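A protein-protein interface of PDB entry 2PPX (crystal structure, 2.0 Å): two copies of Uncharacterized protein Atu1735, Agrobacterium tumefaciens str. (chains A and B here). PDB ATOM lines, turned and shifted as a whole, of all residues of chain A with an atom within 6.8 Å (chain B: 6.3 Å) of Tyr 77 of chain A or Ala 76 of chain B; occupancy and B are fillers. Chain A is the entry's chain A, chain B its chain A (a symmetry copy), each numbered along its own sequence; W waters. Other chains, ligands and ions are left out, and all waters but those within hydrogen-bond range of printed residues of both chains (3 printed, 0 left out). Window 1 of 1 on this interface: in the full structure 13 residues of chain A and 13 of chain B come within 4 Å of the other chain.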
ATOM      1  N   ARG A  52      23.547  16.018 -20.608  1.00  0.00           N
ATOM      2  CA  ARG A  52      24.990  15.805 -20.749  1.00  0.00           C
ATOM      3  C   ARG A  52      25.360  15.074 -22.057  1.00  0.00           C
ATOM      4  O   ARG A  52      26.365  15.410 -22.711  1.00  0.00           O
ATOM      5  CB  ARG A  52      25.531  15.047 -19.542  1.00  0.00           C
ATOM      6  CG  ARG A  52      27.029  14.944 -19.497  1.00  0.00           C
ATOM      7  CD  ARG A  52      27.479  14.399 -18.154  1.00  0.00           C
ATOM      8  NE  ARG A  52      27.206  15.359 -17.085  1.00  0.00           N
ATOM      9  CZ  ARG A  52      27.578  15.203 -15.814  1.00  0.00           C
ATOM     10  NH1 ARG A  52      28.253  14.127 -15.434  1.00  0.00           N
ATOM     11  NH2 ARG A  52      27.266  16.127 -14.923  1.00  0.00           N
ATOM     12  N   TYR A  53      24.530  14.111 -22.444  1.00  0.00           N
ATOM     13  CA  TYR A  53      24.835  13.248 -23.593  1.00  0.00           C
ATOM     14  C   TYR A  53      23.972  13.450 -24.837  1.00  0.00           C
ATOM     15  O   TYR A  53      24.098  12.694 -25.798  1.00  0.00           O
ATOM     16  CB  TYR A  53      24.871  11.764 -23.154  1.00  0.00           C
ATOM     17  CG  TYR A  53      25.973  11.546 -22.146  1.00  0.00           C
ATOM     18  CD1 TYR A  53      27.319  11.680 -22.515  1.00  0.00           C
ATOM     19  CD2 TYR A  53      25.679  11.251 -20.812  1.00  0.00           C
ATOM     20  CE1 TYR A  53      28.346  11.510 -21.579  1.00  0.00           C
ATOM     21  CE2 TYR A  53      26.709  11.052 -19.861  1.00  0.00           C
ATOM     22  CZ  TYR A  53      28.035  11.209 -20.266  1.00  0.00           C
ATOM     23  OH  TYR A  53      29.062  11.059 -19.383  1.00  0.00           O
ATOM     24  N   HIS A  54      23.134  14.493 -24.822  1.00  0.00           N
ATOM     25  CA  HIS A  54      22.303  14.891 -25.966  1.00  0.00           C
ATOM     26  C   HIS A  54      21.382  13.777 -26.456  1.00  0.00           C
ATOM     27  O   HIS A  54      21.275  13.511 -27.659  1.00  0.00           O
ATOM     28  CB  HIS A  54      23.165  15.455 -27.100  1.00  0.00           C
ATOM     29  CG  HIS A  54      24.016  16.623 -26.685  1.00  0.00           C
ATOM     30  ND1 HIS A  54      24.221  17.714 -27.491  1.00  0.00           N
ATOM     31  CD2 HIS A  54      24.657  16.893 -25.525  1.00  0.00           C
ATOM     32  CE1 HIS A  54      24.986  18.593 -26.866  1.00  0.00           C
ATOM     33  NE2 HIS A  54      25.266  18.119 -25.669  1.00  0.00           N
ATOM     34  N   ILE A  55      20.737  13.112 -25.509  1.00  0.00           N
ATOM     35  CA  ILE A  55      19.717  12.104 -25.838  1.00  0.00           C
ATOM     36  C   ILE A  55      18.370  12.671 -25.363  1.00  0.00           C
ATOM     37  O   ILE A  55      18.203  12.945 -24.188  1.00  0.00           O
ATOM     38  CB  ILE A  55      20.009  10.775 -25.171  1.00  0.00           C
ATOM     39  CG1 ILE A  55      21.371  10.210 -25.677  1.00  0.00           C
ATOM     40  CG2 ILE A  55      18.860   9.754 -25.412  1.00  0.00           C
ATOM     41  CD1 ILE A  55      21.923   9.149 -24.796  1.00  0.00           C
ATOM     42  N   TRP A  63      13.761   3.946 -23.769  1.00  0.00           N
ATOM     43  CA  TRP A  63      14.790   2.918 -23.729  1.00  0.00           C
ATOM     44  C   TRP A  63      14.842   2.259 -22.327  1.00  0.00           C
ATOM     45  O   TRP A  63      14.884   1.016 -22.209  1.00  0.00           O
ATOM     46  CB  TRP A  63      16.166   3.455 -24.141  1.00  0.00           C
ATOM     47  CG  TRP A  63      16.267   3.972 -25.549  1.00  0.00           C
ATOM     48  CD1 TRP A  63      15.362   3.792 -26.582  1.00  0.00           C
ATOM     49  CD2 TRP A  63      17.316   4.792 -26.075  1.00  0.00           C
ATOM     50  NE1 TRP A  63      15.810   4.449 -27.696  1.00  0.00           N
ATOM     51  CE2 TRP A  63      17.014   5.039 -27.429  1.00  0.00           C
ATOM     52  CE3 TRP A  63      18.504   5.300 -25.537  1.00  0.00           C
ATOM     53  CZ2 TRP A  63      17.836   5.821 -28.255  1.00  0.00           C
ATOM     54  CZ3 TRP A  63      19.336   6.055 -26.361  1.00  0.00           C
ATOM     55  CH2 TRP A  63      18.979   6.321 -27.703  1.00  0.00           C
ATOM     56  N   ASP A  71      18.749   2.306 -31.703  1.00  0.00           N
ATOM     57  CA  ASP A  71      19.210   1.835 -33.020  1.00  0.00           C
ATOM     58  C   ASP A  71      20.746   1.648 -33.010  1.00  0.00           C
ATOM     59  O   ASP A  71      21.386   1.840 -31.970  1.00  0.00           O
ATOM     60  CB  ASP A  71      18.737   2.781 -34.167  1.00  0.00           C
ATOM     61  CG  ASP A  71      19.424   4.186 -34.153  1.00  0.00           C
ATOM     62  OD1 ASP A  71      20.372   4.488 -33.378  1.00  0.00           O
ATOM     63  OD2 ASP A  71      19.004   5.038 -34.976  1.00  0.00           O
ATOM     64  N   GLN A  72      21.323   1.244 -34.136  1.00  0.00           N
ATOM     65  CA  GLN A  72      22.736   0.808 -34.125  1.00  0.00           C
ATOM     66  C   GLN A  72      23.708   1.939 -33.749  1.00  0.00           C
ATOM     67  O   GLN A  72      24.568   1.720 -32.860  1.00  0.00           O
ATOM     68  CB  GLN A  72      23.165   0.035 -35.399  1.00  0.00           C
ATOM     69  CG  GLN A  72      24.531  -0.689 -35.208  1.00  0.00           C
ATOM     70  CD  GLN A  72      25.139  -1.359 -36.474  1.00  0.00           C
ATOM     71  OE1 GLN A  72      24.628  -1.242 -37.599  1.00  0.00           O
ATOM     72  NE2 GLN A  72      26.239  -2.095 -36.263  1.00  0.00           N
ATOM     73  N   PRO A  73      23.555   3.146 -34.384  1.00  0.00           N
ATOM     74  CA  PRO A  73      24.466   4.260 -33.990  1.00  0.00           C
ATOM     75  C   PRO A  73      24.293   4.617 -32.522  1.00  0.00           C
ATOM     76  O   PRO A  73      25.262   4.897 -31.858  1.00  0.00           O
ATOM     77  CB  PRO A  73      24.016   5.439 -34.900  1.00  0.00           C
ATOM     78  CG  PRO A  73      23.382   4.766 -36.069  1.00  0.00           C
ATOM     79  CD  PRO A  73      22.636   3.583 -35.464  1.00  0.00           C
ATOM     80  N   ALA A  74      23.056   4.595 -32.021  1.00  0.00           N
ATOM     81  CA  ALA A  74      22.841   4.872 -30.584  1.00  0.00           C
ATOM     82  C   ALA A  74      23.481   3.856 -29.636  1.00  0.00           C
ATOM     83  O   ALA A  74      24.012   4.246 -28.581  1.00  0.00           O
ATOM     84  CB  ALA A  74      21.324   5.024 -30.297  1.00  0.00           C
ATOM     85  N   ARG A  75      23.427   2.558 -29.982  1.00  0.00           N
ATOM     86  CA  ARG A  75      24.080   1.548 -29.167  1.00  0.00           C
ATOM     87  C   ARG A  75      25.572   1.762 -29.149  1.00  0.00           C
ATOM     88  O   ARG A  75      26.213   1.610 -28.087  1.00  0.00           O
ATOM     89  CB  ARG A  75      23.793   0.108 -29.650  1.00  0.00           C
ATOM     90  CG  ARG A  75      22.316  -0.267 -29.514  1.00  0.00           C
ATOM     91  CD  ARG A  75      22.111  -1.757 -29.684  1.00  0.00           C
ATOM     92  NE  ARG A  75      22.471  -2.290 -31.017  1.00  0.00           N
ATOM     93  CZ  ARG A  75      21.673  -2.295 -32.098  1.00  0.00           C
ATOM     94  NH1 ARG A  75      20.453  -1.727 -32.094  1.00  0.00           N
ATOM     95  NH2 ARG A  75      22.105  -2.875 -33.212  1.00  0.00           N
ATOM     96  N   ALA A  76      26.140   2.078 -30.324  1.00  0.00           N
ATOM     97  CA  ALA A  76      27.588   2.343 -30.428  1.00  0.00           C
ATOM     98  C   ALA A  76      27.939   3.543 -29.539  1.00  0.00           C
ATOM     99  O   ALA A  76      28.904   3.518 -28.778  1.00  0.00           O
ATOM    100  CB  ALA A  76      27.969   2.593 -31.866  1.00  0.00           C
ATOM    101  N   TYR A  77      27.110   4.583 -29.620  1.00  0.00           N
ATOM    102  CA  TYR A  77      27.304   5.803 -28.814  1.00  0.00           C
ATOM    103  C   TYR A  77      27.277   5.510 -27.297  1.00  0.00           C
ATOM    104  O   TYR A  77      28.096   6.019 -26.546  1.00  0.00           O
ATOM    105  CB  TYR A  77      26.228   6.834 -29.205  1.00  0.00           C
ATOM    106  CG  TYR A  77      26.323   8.149 -28.442  1.00  0.00           C
ATOM    107  CD1 TYR A  77      27.561   8.737 -28.161  1.00  0.00           C
ATOM    108  CD2 TYR A  77      25.167   8.810 -28.038  1.00  0.00           C
ATOM    109  CE1 TYR A  77      27.635   9.925 -27.466  1.00  0.00           C
ATOM    110  CE2 TYR A  77      25.224  10.007 -27.350  1.00  0.00           C
ATOM    111  CZ  TYR A  77      26.449  10.562 -27.072  1.00  0.00           C
ATOM    112  OH  TYR A  77      26.509  11.734 -26.366  1.00  0.00           O
ATOM    113  N   LEU A  78      26.305   4.719 -26.860  1.00  0.00           N
ATOM    114  CA  LEU A  78      26.190   4.289 -25.462  1.00  0.00           C
ATOM    115  C   LEU A  78      27.389   3.513 -24.995  1.00  0.00           C
ATOM    116  O   LEU A  78      27.812   3.650 -23.847  1.00  0.00           O
ATOM    117  CB  LEU A  78      24.924   3.426 -25.249  1.00  0.00           C
ATOM    118  CG  LEU A  78      23.649   4.260 -25.326  1.00  0.00           C
ATOM    119  CD1 LEU A  78      22.390   3.415 -25.359  1.00  0.00           C
ATOM    120  CD2 LEU A  78      23.604   5.322 -24.165  1.00  0.00           C
ATOM    121  N   LYS A  79      27.953   2.700 -25.876  1.00  0.00           N
ATOM    122  CA  LYS A  79      29.206   2.030 -25.542  1.00  0.00           C
ATOM    123  C   LYS A  79      30.366   3.017 -25.319  1.00  0.00           C
ATOM    124  O   LYS A  79      31.186   2.839 -24.404  1.00  0.00           O
ATOM    125  CB  LYS A  79      29.553   0.975 -26.590  1.00  0.00           C
ATOM    126  CG  LYS A  79      30.951   0.374 -26.360  1.00  0.00           C
ATOM    127  CD  LYS A  79      30.907  -1.137 -26.425  1.00  0.00           C
ATOM    128  CE  LYS A  79      32.199  -1.751 -25.875  1.00  0.00           C
ATOM    129  NZ  LYS A  79      32.719  -2.714 -26.882  1.00  0.00           N
ATOM    130  N   ILE A  80      30.430   4.091 -26.118  1.00  0.00           N
ATOM    131  CA  ILE A  80      31.500   5.073 -25.935  1.00  0.00           C
ATOM    132  C   ILE A  80      31.324   5.817 -24.634  1.00  0.00           C
ATOM    133  O   ILE A  80      32.303   6.063 -23.919  1.00  0.00           O
ATOM    134  CB  ILE A  80      31.572   6.134 -27.087  1.00  0.00           C
ATOM    135  CG1 ILE A  80      31.591   5.448 -28.452  1.00  0.00           C
ATOM    136  CG2 ILE A  80      32.799   7.022 -26.875  1.00  0.00           C
ATOM    137  CD1 ILE A  80      32.682   4.456 -28.615  1.00  0.00           C
ATOM    138  N   ILE A  81      30.084   6.185 -24.336  1.00  0.00           N
ATOM    139  CA  ILE A  81      29.767   6.842 -23.058  1.00  0.00           C
ATOM    140  C   ILE A  81      30.245   5.950 -21.899  1.00  0.00           C
ATOM    141  O   ILE A  81      30.942   6.405 -20.990  1.00  0.00           O
ATOM    142  CB  ILE A  81      28.237   7.126 -22.910  1.00  0.00           C
ATOM    143  CG1 ILE A  81      27.771   8.153 -23.947  1.00  0.00           C
ATOM    144  CG2 ILE A  81      27.901   7.578 -21.461  1.00  0.00           C
ATOM    145  CD1 ILE A  81      26.262   8.304 -24.023  1.00  0.00           C
ATOM    146  N   ALA A  82      29.866   4.675 -21.943  1.00  0.00           N
ATOM    147  CA  ALA A  82      30.295   3.706 -20.923  1.00  0.00           C
ATOM    148  C   ALA A  82      31.822   3.616 -20.761  1.00  0.00           C
ATOM    149  O   ALA A  82      32.342   3.582 -19.621  1.00  0.00           O
ATOM    150  CB  ALA A  82      29.701   2.332 -21.222  1.00  0.00           C
ATOM    151  N   THR A  88      33.647  11.806 -23.110  1.00  0.00           N
ATOM    152  CA  THR A  88      32.491  11.974 -23.985  1.00  0.00           C
ATOM    153  C   THR A  88      31.735  13.268 -23.649  1.00  0.00           C
ATOM    154  O   THR A  88      31.428  14.060 -24.539  1.00  0.00           O
ATOM    155  CB  THR A  88      31.557  10.722 -23.975  1.00  0.00           C
ATOM    156  OG1 THR A  88      32.318   9.578 -24.377  1.00  0.00           O
ATOM    157  CG2 THR A  88      30.393  10.900 -24.941  1.00  0.00           C
ATOM    158  N   ALA A  89      31.456  13.472 -22.365  1.00  0.00           N
ATOM    159  CA  ALA A  89      30.740  14.651 -21.903  1.00  0.00           C
ATOM    160  C   ALA A  89      31.508  15.930 -22.256  1.00  0.00           C
ATOM    161  O   ALA A  89      30.912  16.897 -22.716  1.00  0.00           O
ATOM    162  CB  ALA A  89      30.501  14.566 -20.396  1.00  0.00           C
ATOM    163  N   LEU A  92      31.401  17.007 -25.960  1.00  0.00           N
ATOM    164  CA  LEU A  92      30.132  17.615 -26.359  1.00  0.00           C
ATOM    165  C   LEU A  92      29.956  19.060 -25.890  1.00  0.00           C
ATOM    166  O   LEU A  92      29.060  19.757 -26.382  1.00  0.00           O
ATOM    167  CB  LEU A  92      28.940  16.755 -25.902  1.00  0.00           C
ATOM    168  CG  LEU A  92      28.843  15.359 -26.499  1.00  0.00           C
ATOM    169  CD1 LEU A  92      27.703  14.572 -25.837  1.00  0.00           C
ATOM    170  CD2 LEU A  92      28.647  15.425 -28.013  1.00  0.00           C
ATOM    171  N   ASP B  71      19.696  12.097 -36.269  1.00  0.00           N
ATOM    172  CA  ASP B  71      18.941  12.535 -35.083  1.00  0.00           C
ATOM    173  C   ASP B  71      19.915  13.001 -33.975  1.00  0.00           C
ATOM    174  O   ASP B  71      21.133  13.016 -34.188  1.00  0.00           O
ATOM    175  CB  ASP B  71      17.962  11.428 -34.583  1.00  0.00           C
ATOM    176  CG  ASP B  71      18.678  10.179 -33.972  1.00  0.00           C
ATOM    177  OD1 ASP B  71      19.922  10.120 -33.771  1.00  0.00           O
ATOM    178  OD2 ASP B  71      17.955   9.200 -33.658  1.00  0.00           O
ATOM    179  N   GLN B  72      19.389  13.410 -32.827  1.00  0.00           N
ATOM    180  CA  GLN B  72      20.238  14.098 -31.830  1.00  0.00           C
ATOM    181  C   GLN B  72      21.355  13.199 -31.275  1.00  0.00           C
ATOM    182  O   GLN B  72      22.531  13.644 -31.258  1.00  0.00           O
ATOM    183  CB  GLN B  72      19.439  14.830 -30.721  1.00  0.00           C
ATOM    184  CG  GLN B  72      20.336  15.805 -29.904  1.00  0.00           C
ATOM    185  CD  GLN B  72      19.679  16.470 -28.660  1.00  0.00           C
ATOM    186  OE1 GLN B  72      18.539  16.169 -28.269  1.00  0.00           O
ATOM    187  NE2 GLN B  72      20.416  17.410 -28.052  1.00  0.00           N
ATOM    188  N   PRO B  73      21.010  11.936 -30.862  1.00  0.00           N
ATOM    189  CA  PRO B  73      22.099  11.044 -30.366  1.00  0.00           C
ATOM    190  C   PRO B  73      23.131  10.783 -31.450  1.00  0.00           C
ATOM    191  O   PRO B  73      24.303  10.741 -31.161  1.00  0.00           O
ATOM    192  CB  PRO B  73      21.352   9.733 -29.989  1.00  0.00           C
ATOM    193  CG  PRO B  73      19.955  10.180 -29.724  1.00  0.00           C
ATOM    194  CD  PRO B  73      19.697  11.252 -30.776  1.00  0.00           C
ATOM    195  N   ALA B  74      22.689  10.619 -32.700  1.00  0.00           N
ATOM    196  CA  ALA B  74      23.658  10.425 -33.801  1.00  0.00           C
ATOM    197  C   ALA B  74      24.585  11.616 -34.050  1.00  0.00           C
ATOM    198  O   ALA B  74      25.780  11.417 -34.337  1.00  0.00           O
ATOM    199  CB  ALA B  74      22.908  10.021 -35.098  1.00  0.00           C
ATOM    200  N   ARG B  75      24.058  12.848 -33.964  1.00  0.00           N
ATOM    201  CA  ARG B  75      24.898  14.025 -34.114  1.00  0.00           C
ATOM    202  C   ARG B  75      25.923  14.090 -33.010  1.00  0.00           C
ATOM    203  O   ARG B  75      27.095  14.443 -33.265  1.00  0.00           O
ATOM    204  CB  ARG B  75      24.091  15.343 -34.118  1.00  0.00           C
ATOM    205  CG  ARG B  75      23.160  15.451 -35.326  1.00  0.00           C
ATOM    206  CD  ARG B  75      22.628  16.858 -35.485  1.00  0.00           C
ATOM    207  NE  ARG B  75      21.784  17.337 -34.368  1.00  0.00           N
ATOM    208  CZ  ARG B  75      20.468  17.109 -34.229  1.00  0.00           C
ATOM    209  NH1 ARG B  75      19.779  16.328 -35.083  1.00  0.00           N
ATOM    210  NH2 ARG B  75      19.823  17.665 -33.209  1.00  0.00           N
ATOM    211  N   ALA B  76      25.487  13.789 -31.777  1.00  0.00           N
ATOM    212  CA  ALA B  76      26.403  13.786 -30.619  1.00  0.00           C
ATOM    213  C   ALA B  76      27.506  12.747 -30.861  1.00  0.00           C
ATOM    214  O   ALA B  76      28.690  13.011 -30.665  1.00  0.00           O
ATOM    215  CB  ALA B  76      25.639  13.494 -29.352  1.00  0.00           C
ATOM    216  N   TYR B  77      27.096  11.570 -31.332  1.00  0.00           N
ATOM    217  CA  TYR B  77      28.040  10.476 -31.631  1.00  0.00           C
ATOM    218  C   TYR B  77      29.085  10.883 -32.694  1.00  0.00           C
ATOM    219  O   TYR B  77      30.265  10.595 -32.555  1.00  0.00           O
ATOM    220  CB  TYR B  77      27.240   9.237 -32.076  1.00  0.00           C
ATOM    221  CG  TYR B  77      28.105   8.028 -32.411  1.00  0.00           C
ATOM    222  CD1 TYR B  77      29.226   7.702 -31.641  1.00  0.00           C
ATOM    223  CD2 TYR B  77      27.770   7.202 -33.479  1.00  0.00           C
ATOM    224  CE1 TYR B  77      30.004   6.609 -31.957  1.00  0.00           C
ATOM    225  CE2 TYR B  77      28.533   6.096 -33.802  1.00  0.00           C
ATOM    226  CZ  TYR B  77      29.638   5.800 -33.042  1.00  0.00           C
ATOM    227  OH  TYR B  77      30.411   4.721 -33.377  1.00  0.00           O
ATOM    228  N   LEU B  78      28.628  11.515 -33.769  1.00  0.00           N
ATOM    229  CA  LEU B  78      29.503  12.029 -34.828  1.00  0.00           C
ATOM    230  C   LEU B  78      30.485  13.048 -34.323  1.00  0.00           C
ATOM    231  O   LEU B  78      31.631  13.085 -34.773  1.00  0.00           O
ATOM    232  CB  LEU B  78      28.675  12.660 -35.973  1.00  0.00           C
ATOM    233  CG  LEU B  78      27.941  11.602 -36.791  1.00  0.00           C
ATOM    234  CD1 LEU B  78      26.941  12.197 -37.765  1.00  0.00           C
ATOM    235  CD2 LEU B  78      28.961  10.649 -37.518  1.00  0.00           C
ATOM    236  N   LYS B  79      30.056  13.875 -33.382  1.00  0.00           N
ATOM    237  CA  LYS B  79      30.995  14.789 -32.739  1.00  0.00           C
ATOM    238  C   LYS B  79      32.096  14.053 -31.955  1.00  0.00           C
ATOM    239  O   LYS B  79      33.271  14.452 -31.981  1.00  0.00           O
ATOM    240  CB  LYS B  79      30.257  15.800 -31.866  1.00  0.00           C
ATOM    241  CG  LYS B  79      31.227  16.664 -31.041  1.00  0.00           C
ATOM    242  CD  LYS B  79      30.873  18.131 -31.153  1.00  0.00           C
ATOM    243  CE  LYS B  79      32.008  19.015 -30.622  1.00  0.00           C
ATOM    244  NZ  LYS B  79      31.429  19.971 -29.642  1.00  0.00           N
ATOM    245  N   ILE B  80      31.748  12.947 -31.283  1.00  0.00           N
ATOM    246  CA  ILE B  80      32.759  12.197 -30.539  1.00  0.00           C
ATOM    247  C   ILE B  80      33.739  11.542 -31.482  1.00  0.00           C
ATOM    248  O   ILE B  80      34.948  11.539 -31.222  1.00  0.00           O
ATOM    249  CB  ILE B  80      32.154  11.076 -29.624  1.00  0.00           C
ATOM    250  CG1 ILE B  80      31.036  11.640 -28.749  1.00  0.00           C
ATOM    251  CG2 ILE B  80      33.272  10.449 -28.792  1.00  0.00           C
ATOM    252  CD1 ILE B  80      31.445  12.798 -27.918  1.00  0.00           C
ATOM    253  N   ILE B  81      33.217  10.978 -32.565  1.00  0.00           N
ATOM    254  CA  ILE B  81      34.072  10.381 -33.603  1.00  0.00           C
ATOM    255  C   ILE B  81      35.072  11.436 -34.103  1.00  0.00           C
ATOM    256  O   ILE B  81      36.278  11.193 -34.165  1.00  0.00           O
ATOM    257  CB  ILE B  81      33.235   9.833 -34.805  1.00  0.00           C
ATOM    258  CG1 ILE B  81      32.357   8.657 -34.367  1.00  0.00           C
ATOM    259  CG2 ILE B  81      34.165   9.448 -35.990  1.00  0.00           C
ATOM    260  CD1 ILE B  81      31.344   8.227 -35.414  1.00  0.00           C
ATOM    261  N   LEU B  92      34.865   0.485 -29.620  1.00  0.00           N
ATOM    262  CA  LEU B  92      33.856  -0.376 -30.235  1.00  0.00           C
ATOM    263  C   LEU B  92      34.352  -1.785 -30.562  1.00  0.00           C
ATOM    264  O   LEU B  92      33.533  -2.673 -30.834  1.00  0.00           O
ATOM    265  CB  LEU B  92      33.258   0.286 -31.490  1.00  0.00           C
ATOM    266  CG  LEU B  92      32.499   1.587 -31.274  1.00  0.00           C
ATOM    267  CD1 LEU B  92      32.099   2.202 -32.622  1.00  0.00           C
ATOM    268  CD2 LEU B  92      31.270   1.362 -30.395  1.00  0.00           C
HETATM  269  O   HOH W   1      23.633  16.308 -30.478  1.00  0.00           O
HETATM  270  O   HOH W   2      21.285   7.430 -33.068  1.00  0.00           O
HETATM  271  O   HOH W   3      23.961   7.728 -31.875  1.00  0.00           O
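Of the 12 printed residues of chain B, 6 touch a printed residue of chain A.
Hydrophobic or aromatic side chains of chain B that line the printed part of chain A: Ala 76, Tyr 77, Ile 80 and Leu 92.
Of the 20 printed residues of chain A, 8 touch a printed residue of chain B.
Printed residues of chain A that touch a printed residue of chain B: Tyr 53, His 54, Pro 73, Ala 76, Tyr 77, Ile 80, Thr 88 and Leu 92.
Hydrophobic or aromatic side chains of chain A that line the printed part of chain B: His 54, Ala 76, Tyr 77, Ile 80 and Leu 92.
Among the printed residues, no Asp or Glu carboxylate lies within 4 Å of a Lys or Arg side-chain nitrogen of the other chain.
Water W1 lies within hydrogen-bond range of the backbone carbonyl oxygen (O) of Gln 72 of chain B (3.0 Å), a ring nitrogen (ND1) of His 54 of chain A (3.4 Å) and the backbone NH (N) of Ala 76 of chain B (3.4 Å).
Water W2 bridges OD1 of Asp 71 of chain A (3.1 Å) and OD1 of Asp 71 of chain B (3.1 Å).
Water W3 lies within hydrogen-bond range of the backbone carbonyl oxygen of Pro 73 of chain A, the backbone carbonyl oxygen of Pro 73 of chain B, the backbone NH of Ala 74 of chain A and the backbone NH of Ala 74 of chain B.
Among the printed residues, pairs that only touch across the chains: His 54 of chain A with Gln 72 of chain B (3.3 Å), Tyr 77 of chain A with Ala 76 of chain B (3.6 Å), Ala 76 of chain A with Tyr 77 of chain B (3.6 Å), His 54 of chain A with Pro 73 of chain B (3.6 Å), Ala 76 of chain A with Leu 92 of chain B (3.6 Å), Leu 92 of chain A with Ala 76 of chain B (3.6 Å), Thr 88 of chain A with Ile 80 of chain B (3.6 Å), Tyr 77 of chain A with Pro 73 of chain B (3.8 Å), Pro 73 of chain A with Tyr 77 of chain B (3.8 Å), Ile 80 of chain A with Leu 92 of chain B (3.8 Å), Leu 92 of chain A with Ile 80 of chain B (3.8 Å), His 54 of chain A with Ala 76 of chain B (3.9 Å), Tyr 77 of chain A with Tyr 77 of chain B (3.9 Å), Ile 80 of chain A with Ile 80 of chain B (3.96 Å) and Tyr 53 of chain A with Ala 76 of chain B (3.96 Å).
The backbone carbonyl oxygen (O) of Tyr 53 of chain A is in hydrogen-bond range of the side-chain hydroxyl (OH) of Tyr 77 of chain A (2.7 Å).
Printed residues of chain B within 4 Å of Tyr 77 of chain A: Pro 73, Ala 76 and Tyr 77.
Of the printed residues of chain A, Tyr 77 of chain B touches Pro 73 (3.8 Å), Ala 76 (3.6 Å) and Tyr 77 (3.9 Å).
Of the printed residues of chain B, Thr 88 of chain A touches Ile 80.
Printed residues of chain A within 4 Å of Gln 72 of chain B: His 54.
The nearest printed residue of chain B that does not touch Tyr 77 of chain A is Ile 80 of chain B (4.02 Å).
The nearest residue of chain A that does not touch Ala 76 of chain B is Ile 55 of chain A (6.2 Å).
Pro 73 of chain A touches Tyr 77 of chain B, and with the chains exchanged Tyr 77 of chain A touches Pro 73 of chain B.
Ala 76 of chain A touches Tyr 77 of chain B, and with the chains exchanged Tyr 77 of chain A touches Ala 76 of chain B.
Ala 76 of chain A touches Leu 92 of chain B, and with the chains exchanged Leu 92 of chain A touches Ala 76 of chain B.
Ile 80 of chain A touches Leu 92 of chain B, and with the chains exchanged Leu 92 of chain A touches Ile 80 of chain B.
12 positions are printed for both chains.
Of the 15 pairs that touch across the chains among the printed residues, 10 have their exchanged pair printed and touching as well.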
